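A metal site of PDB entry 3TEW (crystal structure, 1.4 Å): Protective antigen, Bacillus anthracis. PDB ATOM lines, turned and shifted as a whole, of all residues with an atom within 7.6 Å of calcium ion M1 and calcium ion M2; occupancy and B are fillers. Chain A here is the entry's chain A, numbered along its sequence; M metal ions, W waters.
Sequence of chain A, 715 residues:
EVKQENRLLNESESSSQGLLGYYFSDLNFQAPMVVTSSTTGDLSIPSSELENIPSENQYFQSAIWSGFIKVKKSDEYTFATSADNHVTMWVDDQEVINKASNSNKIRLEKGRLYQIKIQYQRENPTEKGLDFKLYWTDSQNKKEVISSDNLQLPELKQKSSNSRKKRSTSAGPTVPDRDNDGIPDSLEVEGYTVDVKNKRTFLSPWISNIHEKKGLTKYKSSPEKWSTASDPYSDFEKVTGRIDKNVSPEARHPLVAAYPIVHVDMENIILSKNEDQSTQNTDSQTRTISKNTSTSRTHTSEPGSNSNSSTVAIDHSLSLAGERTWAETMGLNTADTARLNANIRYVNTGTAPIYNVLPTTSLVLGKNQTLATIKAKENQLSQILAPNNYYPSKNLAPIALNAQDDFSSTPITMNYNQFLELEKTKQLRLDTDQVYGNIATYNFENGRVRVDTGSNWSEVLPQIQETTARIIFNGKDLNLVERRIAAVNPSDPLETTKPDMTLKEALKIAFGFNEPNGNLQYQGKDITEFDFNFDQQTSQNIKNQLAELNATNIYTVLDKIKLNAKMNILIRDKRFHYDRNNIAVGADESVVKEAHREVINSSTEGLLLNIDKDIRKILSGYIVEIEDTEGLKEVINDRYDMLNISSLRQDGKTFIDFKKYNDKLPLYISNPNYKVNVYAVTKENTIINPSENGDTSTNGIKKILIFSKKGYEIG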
ATOM      1  N   TYR A  22       8.425  -5.005  -5.866  1.00  0.00           N
ATOM      2  CA  TYR A  22       7.748  -4.560  -7.060  1.00  0.00           C
ATOM      3  C   TYR A  22       8.760  -4.740  -8.204  1.00  0.00           C
ATOM      4  O   TYR A  22       9.862  -4.206  -8.119  1.00  0.00           O
ATOM      5  CB  TYR A  22       7.375  -3.091  -6.932  1.00  0.00           C
ATOM      6  CG  TYR A  22       6.414  -2.817  -5.795  1.00  0.00           C
ATOM      7  CD1 TYR A  22       6.861  -2.640  -4.494  1.00  0.00           C
ATOM      8  CD2 TYR A  22       5.045  -2.770  -6.024  1.00  0.00           C
ATOM      9  CE1 TYR A  22       5.973  -2.407  -3.467  1.00  0.00           C
ATOM     10  CE2 TYR A  22       4.160  -2.533  -5.011  1.00  0.00           C
ATOM     11  CZ  TYR A  22       4.623  -2.351  -3.744  1.00  0.00           C
ATOM     12  OH  TYR A  22       3.740  -2.115  -2.708  1.00  0.00           O
ATOM     13  N   PRO A 176       3.843   4.630  -6.860  1.00  0.00           N
ATOM     14  CA  PRO A 176       2.615   5.358  -6.545  1.00  0.00           C
ATOM     15  C   PRO A 176       1.613   4.421  -5.919  1.00  0.00           C
ATOM     16  O   PRO A 176       1.179   3.445  -6.540  1.00  0.00           O
ATOM     17  CB  PRO A 176       2.131   5.829  -7.921  1.00  0.00           C
ATOM     18  CG  PRO A 176       3.364   5.889  -8.748  1.00  0.00           C
ATOM     19  CD  PRO A 176       4.200   4.733  -8.288  1.00  0.00           C
ATOM     20  N   ASP A 177       1.260   4.722  -4.675  1.00  0.00           N
ATOM     21  CA  ASP A 177       0.357   3.902  -3.889  1.00  0.00           C
ATOM     22  C   ASP A 177      -0.350   4.864  -2.926  1.00  0.00           C
ATOM     23  O   ASP A 177      -0.061   4.882  -1.730  1.00  0.00           O
ATOM     24  CB  ASP A 177       1.155   2.835  -3.117  1.00  0.00           C
ATOM     25  CG  ASP A 177       0.271   1.909  -2.290  1.00  0.00           C
ATOM     26  OD1 ASP A 177      -0.928   1.831  -2.588  1.00  0.00           O
ATOM     27  OD2 ASP A 177       0.773   1.252  -1.364  1.00  0.00           O
ATOM     28  N   ARG A 178      -1.263   5.644  -3.498  1.00  0.00           N
ATOM     29  CA  ARG A 178      -1.915   6.753  -2.792  1.00  0.00           C
ATOM     30  C   ARG A 178      -2.590   6.325  -1.466  1.00  0.00           C
ATOM     31  O   ARG A 178      -2.651   7.090  -0.506  1.00  0.00           O
ATOM     32  CB  ARG A 178      -2.927   7.435  -3.741  1.00  0.00           C
ATOM     33  CG  ARG A 178      -2.307   8.090  -4.994  1.00  0.00           C
ATOM     34  CD  ARG A 178      -3.340   8.405  -6.076  1.00  0.00           C
ATOM     35  NE  ARG A 178      -3.992   9.701  -5.925  1.00  0.00           N
ATOM     36  CZ  ARG A 178      -3.373  10.853  -6.155  1.00  0.00           C
ATOM     37  NH1 ARG A 178      -2.108  10.840  -6.511  1.00  0.00           N
ATOM     38  NH2 ARG A 178      -4.005  12.010  -6.000  1.00  0.00           N
ATOM     39  N   ASP A 179      -3.121   5.116  -1.408  1.00  0.00           N
ATOM     40  CA  ASP A 179      -3.866   4.690  -0.207  1.00  0.00           C
ATOM     41  C   ASP A 179      -3.072   3.752   0.707  1.00  0.00           C
ATOM     42  O   ASP A 179      -3.595   3.226   1.697  1.00  0.00           O
ATOM     43  CB  ASP A 179      -5.191   4.031  -0.618  1.00  0.00           C
ATOM     44  CG  ASP A 179      -4.993   2.859  -1.575  1.00  0.00           C
ATOM     45  OD1 ASP A 179      -3.857   2.352  -1.713  1.00  0.00           O
ATOM     46  OD2 ASP A 179      -5.981   2.445  -2.189  1.00  0.00           O
ATOM     47  N   ASN A 180      -1.805   3.545   0.368  1.00  0.00           N
ATOM     48  CA  ASN A 180      -0.927   2.723   1.205  1.00  0.00           C
ATOM     49  C   ASN A 180      -1.398   1.288   1.456  1.00  0.00           C
ATOM     50  O   ASN A 180      -1.063   0.701   2.489  1.00  0.00           O
ATOM     51  CB  ASN A 180      -0.630   3.392   2.546  1.00  0.00           C
ATOM     52  CG  ASN A 180       0.706   2.958   3.121  1.00  0.00           C
ATOM     53  OD1 ASN A 180       1.686   2.829   2.390  1.00  0.00           O
ATOM     54  ND2 ASN A 180       0.742   2.723   4.419  1.00  0.00           N
ATOM     55  N   ASP A 181      -2.179   0.712   0.540  1.00  0.00           N
ATOM     56  CA  ASP A 181      -2.536  -0.687   0.719  1.00  0.00           C
ATOM     57  C   ASP A 181      -1.472  -1.638   0.179  1.00  0.00           C
ATOM     58  O   ASP A 181      -1.494  -2.811   0.525  1.00  0.00           O
ATOM     59  CB  ASP A 181      -3.953  -1.033   0.214  1.00  0.00           C
ATOM     60  CG  ASP A 181      -4.172  -0.757  -1.287  1.00  0.00           C
ATOM     61  OD1 ASP A 181      -3.192  -0.661  -2.057  1.00  0.00           O
ATOM     62  OD2 ASP A 181      -5.369  -0.673  -1.713  1.00  0.00           O
ATOM     63  N   GLY A 182      -0.534  -1.126  -0.599  1.00  0.00           N
ATOM     64  CA  GLY A 182       0.462  -2.005  -1.203  1.00  0.00           C
ATOM     65  C   GLY A 182       0.280  -2.240  -2.691  1.00  0.00           C
ATOM     66  O   GLY A 182       1.254  -2.531  -3.397  1.00  0.00           O
ATOM     67  N   ILE A 183      -0.928  -2.097  -3.221  1.00  0.00           N
ATOM     68  CA  ILE A 183      -1.141  -2.315  -4.649  1.00  0.00           C
ATOM     69  C   ILE A 183      -0.954  -0.990  -5.383  1.00  0.00           C
ATOM     70  O   ILE A 183      -1.590   0.008  -5.042  1.00  0.00           O
ATOM     71  CB  ILE A 183      -2.577  -2.809  -4.951  1.00  0.00           C
ATOM     72  CG1 ILE A 183      -2.962  -4.006  -4.063  1.00  0.00           C
ATOM     73  CG2 ILE A 183      -2.687  -3.168  -6.432  1.00  0.00           C
ATOM     74  CD1 ILE A 183      -4.430  -4.360  -4.186  1.00  0.00           C
ATOM     75  N   PRO A 184      -0.047  -0.957  -6.376  1.00  0.00           N
ATOM     76  CA  PRO A 184       0.209   0.291  -7.092  1.00  0.00           C
ATOM     77  C   PRO A 184      -1.051   0.892  -7.696  1.00  0.00           C
ATOM     78  O   PRO A 184      -1.916   0.123  -8.127  1.00  0.00           O
ATOM     79  CB  PRO A 184       1.153  -0.153  -8.209  1.00  0.00           C
ATOM     80  CG  PRO A 184       1.933  -1.286  -7.596  1.00  0.00           C
ATOM     81  CD  PRO A 184       0.881  -2.033  -6.796  1.00  0.00           C
ATOM     82  N   ASP A 185      -1.138   2.224  -7.721  1.00  0.00           N
ATOM     83  CA  ASP A 185      -2.308   2.946  -8.231  1.00  0.00           C
ATOM     84  C   ASP A 185      -2.734   2.357  -9.582  1.00  0.00           C
ATOM     85  O   ASP A 185      -3.911   2.066  -9.800  1.00  0.00           O
ATOM     86  CB  ASP A 185      -2.004   4.434  -8.511  1.00  0.00           C
ATOM     87  CG  ASP A 185      -1.608   5.261  -7.279  1.00  0.00           C
ATOM     88  OD1 ASP A 185      -1.742   4.822  -6.114  1.00  0.00           O
ATOM     89  OD2 ASP A 185      -1.160   6.415  -7.487  1.00  0.00           O
ATOM     90  N   SER A 186      -1.781   2.224 -10.509  1.00  0.00           N
ATOM     91  CA  SER A 186      -2.080   1.827 -11.876  1.00  0.00           C
ATOM     92  C   SER A 186      -2.707   0.439 -11.986  1.00  0.00           C
ATOM     93  O   SER A 186      -3.587   0.209 -12.826  1.00  0.00           O
ATOM     94  CB  SER A 186      -0.844   1.939 -12.777  1.00  0.00           C
ATOM     95  OG  SER A 186       0.187   1.049 -12.379  1.00  0.00           O
ATOM     96  N   GLU A 188      -4.520  -1.051  -9.657  1.00  0.00           N
ATOM     97  CA  GLU A 188      -5.871  -1.022  -9.094  1.00  0.00           C
ATOM     98  C   GLU A 188      -6.859  -0.477 -10.111  1.00  0.00           C
ATOM     99  O   GLU A 188      -7.982  -0.960 -10.224  1.00  0.00           O
ATOM    100  CB  GLU A 188      -5.903  -0.175  -7.846  1.00  0.00           C
ATOM    101  CG  GLU A 188      -5.150  -0.808  -6.712  1.00  0.00           C
ATOM    102  CD  GLU A 188      -5.613  -0.264  -5.368  1.00  0.00           C
ATOM    103  OE1 GLU A 188      -6.701  -0.663  -4.926  1.00  0.00           O
ATOM    104  OE2 GLU A 188      -4.930   0.565  -4.761  1.00  0.00           O
ATOM    105  N   TYR A 192      -6.048  -6.212 -12.188  1.00  0.00           N
ATOM    106  CA  TYR A 192      -4.970  -7.084 -11.750  1.00  0.00           C
ATOM    107  C   TYR A 192      -5.481  -8.474 -11.420  1.00  0.00           C
ATOM    108  O   TYR A 192      -6.674  -8.699 -11.225  1.00  0.00           O
ATOM    109  CB  TYR A 192      -4.228  -6.519 -10.541  1.00  0.00           C
ATOM    110  CG  TYR A 192      -5.084  -6.174  -9.327  1.00  0.00           C
ATOM    111  CD1 TYR A 192      -5.818  -4.989  -9.289  1.00  0.00           C
ATOM    112  CD2 TYR A 192      -5.122  -7.004  -8.213  1.00  0.00           C
ATOM    113  CE1 TYR A 192      -6.543  -4.640  -8.183  1.00  0.00           C
ATOM    114  CE2 TYR A 192      -5.868  -6.663  -7.082  1.00  0.00           C
ATOM    115  CZ  TYR A 192      -6.578  -5.477  -7.091  1.00  0.00           C
ATOM    116  OH  TYR A 192      -7.314  -5.137  -5.989  1.00  0.00           O
ATOM    117  N   SER A 221      -9.917  -2.070  -8.166  1.00  0.00           N
ATOM    118  CA  SER A 221     -10.219  -1.495  -6.860  1.00  0.00           C
ATOM    119  C   SER A 221      -9.866  -0.006  -6.898  1.00  0.00           C
ATOM    120  O   SER A 221      -9.329   0.481  -7.897  1.00  0.00           O
ATOM    121  CB  SER A 221      -9.500  -2.277  -5.761  1.00  0.00           C
ATOM    122  OG  SER A 221      -8.121  -2.518  -6.057  1.00  0.00           O
ATOM    123  N   SER A 222     -10.273   0.747  -5.877  1.00  0.00           N
ATOM    124  CA  SER A 222      -9.918   2.168  -5.874  1.00  0.00           C
ATOM    125  C   SER A 222      -8.485   2.373  -5.374  1.00  0.00           C
ATOM    126  O   SER A 222      -8.117   1.869  -4.300  1.00  0.00           O
ATOM    127  CB  SER A 222     -10.847   2.963  -4.967  1.00  0.00           C
ATOM    128  OG  SER A 222     -10.297   4.272  -4.828  1.00  0.00           O
ATOM    129  N   PRO A 223      -7.683   3.135  -6.136  1.00  0.00           N
ATOM    130  CA  PRO A 223      -6.324   3.459  -5.710  1.00  0.00           C
ATOM    131  C   PRO A 223      -6.298   4.499  -4.581  1.00  0.00           C
ATOM    132  O   PRO A 223      -5.223   4.820  -4.083  1.00  0.00           O
ATOM    133  CB  PRO A 223      -5.702   4.067  -6.975  1.00  0.00           C
ATOM    134  CG  PRO A 223      -6.871   4.725  -7.656  1.00  0.00           C
ATOM    135  CD  PRO A 223      -8.031   3.776  -7.421  1.00  0.00           C
ATOM    136  N   GLU A 224      -7.460   5.012  -4.195  1.00  0.00           N
ATOM    137  CA  GLU A 224      -7.563   6.012  -3.138  1.00  0.00           C
ATOM    138  C   GLU A 224      -8.308   5.527  -1.886  1.00  0.00           C
ATOM    139  O   GLU A 224      -8.459   6.271  -0.907  1.00  0.00           O
ATOM    140  CB  GLU A 224      -8.198   7.274  -3.677  1.00  0.00           C
ATOM    141  CG  GLU A 224      -7.228   7.936  -4.678  1.00  0.00           C
ATOM    142  CD  GLU A 224      -7.659   9.277  -5.186  1.00  0.00           C
ATOM    143  OE1 GLU A 224      -8.525   9.907  -4.549  1.00  0.00           O
ATOM    144  OE2 GLU A 224      -7.104   9.707  -6.226  1.00  0.00           O
ATOM    145  N   LYS A 225      -8.752   4.285  -1.914  1.00  0.00           N
ATOM    146  CA  LYS A 225      -9.344   3.651  -0.739  1.00  0.00           C
ATOM    147  C   LYS A 225      -8.535   2.430  -0.329  1.00  0.00           C
ATOM    148  O   LYS A 225      -8.439   1.461  -1.122  1.00  0.00           O
ATOM    149  CB  LYS A 225     -10.792   3.242  -0.999  1.00  0.00           C
ATOM    150  CG  LYS A 225     -11.691   4.408  -1.428  1.00  0.00           C
ATOM    151  CD  LYS A 225     -13.139   3.968  -1.644  1.00  0.00           C
ATOM    152  CE  LYS A 225     -13.780   3.639  -0.281  1.00  0.00           C
ATOM    153  NZ  LYS A 225     -15.127   3.103  -0.362  1.00  0.00           N
ATOM    154  N   TRP A 226      -8.032   2.448   0.880  1.00  0.00           N
ATOM    155  CA  TRP A 226      -7.253   1.346   1.449  1.00  0.00           C
ATOM    156  C   TRP A 226      -8.109   0.073   1.420  1.00  0.00           C
ATOM    157  O   TRP A 226      -7.628  -1.001   1.031  1.00  0.00           O
ATOM    158  CB  TRP A 226      -6.818   1.742   2.848  1.00  0.00           C
ATOM    159  CG  TRP A 226      -6.039   0.749   3.622  1.00  0.00           C
ATOM    160  CD1 TRP A 226      -4.667   0.553   3.585  1.00  0.00           C
ATOM    161  CD2 TRP A 226      -6.555  -0.149   4.569  1.00  0.00           C
ATOM    162  NE1 TRP A 226      -4.335  -0.440   4.485  1.00  0.00           N
ATOM    163  CE2 TRP A 226      -5.479  -0.895   5.091  1.00  0.00           C
ATOM    164  CE3 TRP A 226      -7.852  -0.421   5.033  1.00  0.00           C
ATOM    165  CZ2 TRP A 226      -5.651  -1.897   6.056  1.00  0.00           C
ATOM    166  CZ3 TRP A 226      -8.024  -1.423   5.998  1.00  0.00           C
ATOM    167  CH2 TRP A 226      -6.927  -2.148   6.490  1.00  0.00           C
ATOM    168  N   SER A 227      -9.383   0.206   1.783  1.00  0.00           N
ATOM    169  CA  SER A 227     -10.389  -0.863   1.581  1.00  0.00           C
ATOM    170  C   SER A 227     -11.453  -0.295   0.692  1.00  0.00           C
ATOM    171  O   SER A 227     -12.162   0.636   1.103  1.00  0.00           O
ATOM    172  CB  SER A 227     -11.022  -1.321   2.905  1.00  0.00           C
ATOM    173  OG  SER A 227     -12.111  -2.201   2.637  1.00  0.00           O
ATOM    174  N   THR A 228     -11.543  -0.807  -0.523  1.00  0.00           N
ATOM    175  CA  THR A 228     -12.499  -0.246  -1.481  1.00  0.00           C
ATOM    176  C   THR A 228     -13.944  -0.418  -1.011  1.00  0.00           C
ATOM    177  O   THR A 228     -14.789   0.419  -1.355  1.00  0.00           O
ATOM    178  CB  THR A 228     -12.230  -0.791  -2.894  1.00  0.00           C
ATOM    179  OG1 THR A 228     -10.955  -0.299  -3.312  1.00  0.00           O
ATOM    180  CG2 THR A 228     -13.280  -0.273  -3.882  1.00  0.00           C
ATOM    181  N   SER A 234      -7.747  -4.512   3.990  1.00  0.00           N
ATOM    182  CA  SER A 234      -7.303  -3.764   2.818  1.00  0.00           C
ATOM    183  C   SER A 234      -7.448  -4.566   1.536  1.00  0.00           C
ATOM    184  O   SER A 234      -7.579  -5.809   1.527  1.00  0.00           O
ATOM    185  CB  SER A 234      -5.841  -3.328   2.969  1.00  0.00           C
ATOM    186  OG  SER A 234      -4.978  -4.286   2.365  1.00  0.00           O
ATOM    187  N   ASP A 235      -7.438  -3.836   0.429  1.00  0.00           N
ATOM    188  CA  ASP A 235      -7.559  -4.486  -0.884  1.00  0.00           C
ATOM    189  C   ASP A 235      -6.448  -5.519  -1.064  1.00  0.00           C
ATOM    190  O   ASP A 235      -6.673  -6.626  -1.610  1.00  0.00           O
ATOM    191  CB  ASP A 235      -7.528  -3.422  -1.977  1.00  0.00           C
ATOM    192  CG  ASP A 235      -8.720  -2.472  -1.917  1.00  0.00           C
ATOM    193  OD1 ASP A 235      -9.790  -2.824  -1.357  1.00  0.00           O
ATOM    194  OD2 ASP A 235      -8.556  -1.358  -2.487  1.00  0.00           O
ATOM    195  N   PHE A 236      -5.254  -5.164  -0.592  1.00  0.00           N
ATOM    196  CA  PHE A 236      -4.075  -6.047  -0.651  1.00  0.00           C
ATOM    197  C   PHE A 236      -4.165  -7.239   0.298  1.00  0.00           C
ATOM    198  O   PHE A 236      -3.874  -8.385  -0.096  1.00  0.00           O
ATOM    199  CB  PHE A 236      -2.829  -5.198  -0.379  1.00  0.00           C
ATOM    200  CG  PHE A 236      -1.531  -5.963  -0.429  1.00  0.00           C
ATOM    201  CD1 PHE A 236      -0.938  -6.272  -1.638  1.00  0.00           C
ATOM    202  CD2 PHE A 236      -0.888  -6.317   0.747  1.00  0.00           C
ATOM    203  CE1 PHE A 236       0.288  -6.940  -1.688  1.00  0.00           C
ATOM    204  CE2 PHE A 236       0.347  -6.980   0.714  1.00  0.00           C
ATOM    205  CZ  PHE A 236       0.932  -7.291  -0.526  1.00  0.00           C
ATOM    206  N   PRO A 254     -11.920  -7.315  -3.405  1.00  0.00           N
ATOM    207  CA  PRO A 254     -11.914  -5.943  -2.871  1.00  0.00           C
ATOM    208  C   PRO A 254     -13.228  -5.215  -3.082  1.00  0.00           C
ATOM    209  O   PRO A 254     -13.429  -4.184  -2.390  1.00  0.00           O
ATOM    210  CB  PRO A 254     -10.788  -5.266  -3.680  1.00  0.00           C
ATOM    211  CG  PRO A 254      -9.840  -6.397  -3.979  1.00  0.00           C
ATOM    212  CD  PRO A 254     -10.766  -7.564  -4.291  1.00  0.00           C
HETATM  213 CA    CA M   1      -2.960   1.161  -3.548  1.00  0.00          CA
HETATM  214 CA    CA M   2      -7.039   0.445  -2.775  1.00  0.00          CA
HETATM  215  O   HOH W   1      -3.259   3.273  -4.725  1.00  0.00           O
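Of the 26 residues printed, 6 come within 4 Å of calcium ion M2. Along chain A the residues within 4 Å of calcium ion M2 span positions 179 to 235.
O of Ile 183 binds calcium ion M1 (2.3 Å). OD1 of Asp 177 is bound to calcium ion M1 (2.3 Å). OD1 of Asp 179 is bound to calcium ion M1, 2.4 Å away. Calcium ion M1 is bound by the side-chain carboxylate (OD1) of Asp 181 (2.4 Å). The side-chain carboxylate (OE2) of Glu 188 binds calcium ion M1. Calcium ion M1 is bound by water W1, 2.4 Å away.
The backbone NH (N) of Lys 225 is in hydrogen-bond range of the side-chain hydroxyl (OG) of Ser 222 (3.3 Å). The backbone NH (N) of Glu 224 is in hydrogen-bond range of the side-chain hydroxyl (OG) of Ser 222 (3.0 Å). The side-chain amino group of Lys 225 sits at hydrogen-bond distance from the backbone carbonyl oxygen of Thr 228. N of Ser 221 lies within hydrogen-bond range of O of Glu 188, at 3.0 Å. N of Thr 228 sits at hydrogen-bond distance from OD1 of Asp 235 (2.8 Å). N of Gly 182 lies within hydrogen-bond range of OD2 of Asp 177. The backbone NH (N) of Ser 222 is in hydrogen-bond range of the side-chain hydroxyl (OG1) of Thr 228. N of Asp 177 lies close to OD1 of Asp 185 (3.3 Å).
Five residues have an atom within 4 Å of calcium ion M1: Asp 177, Asp 179, Asp 181, Ile 183 and Glu 188.
Water W1 lies within hydrogen-bond range of OD1 of Asp 185 (2.6 Å), O of Pro 223 (2.6 Å) and N of Arg 178 (3.3 Å).
Calcium ion M2 is bound by the side-chain carboxylate (OD2) of Asp 181 (2.3 Å), the side-chain carboxylate (OD2) of Asp 179 (2.3 Å), the backbone carbonyl oxygen (O) of Ser 222 (2.3 Å), the side-chain carboxylate (OD2) of Asp 235 (2.4 Å), the backbone carbonyl oxygen (O) of Lys 225 (2.4 Å), the side-chain carboxylate (OE1) of Glu 188 (2.4 Å) and the side-chain carboxylate (OE2) of Glu 188 (2.9 Å). Calcium ion M2 has seven donor atoms within binding distance.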
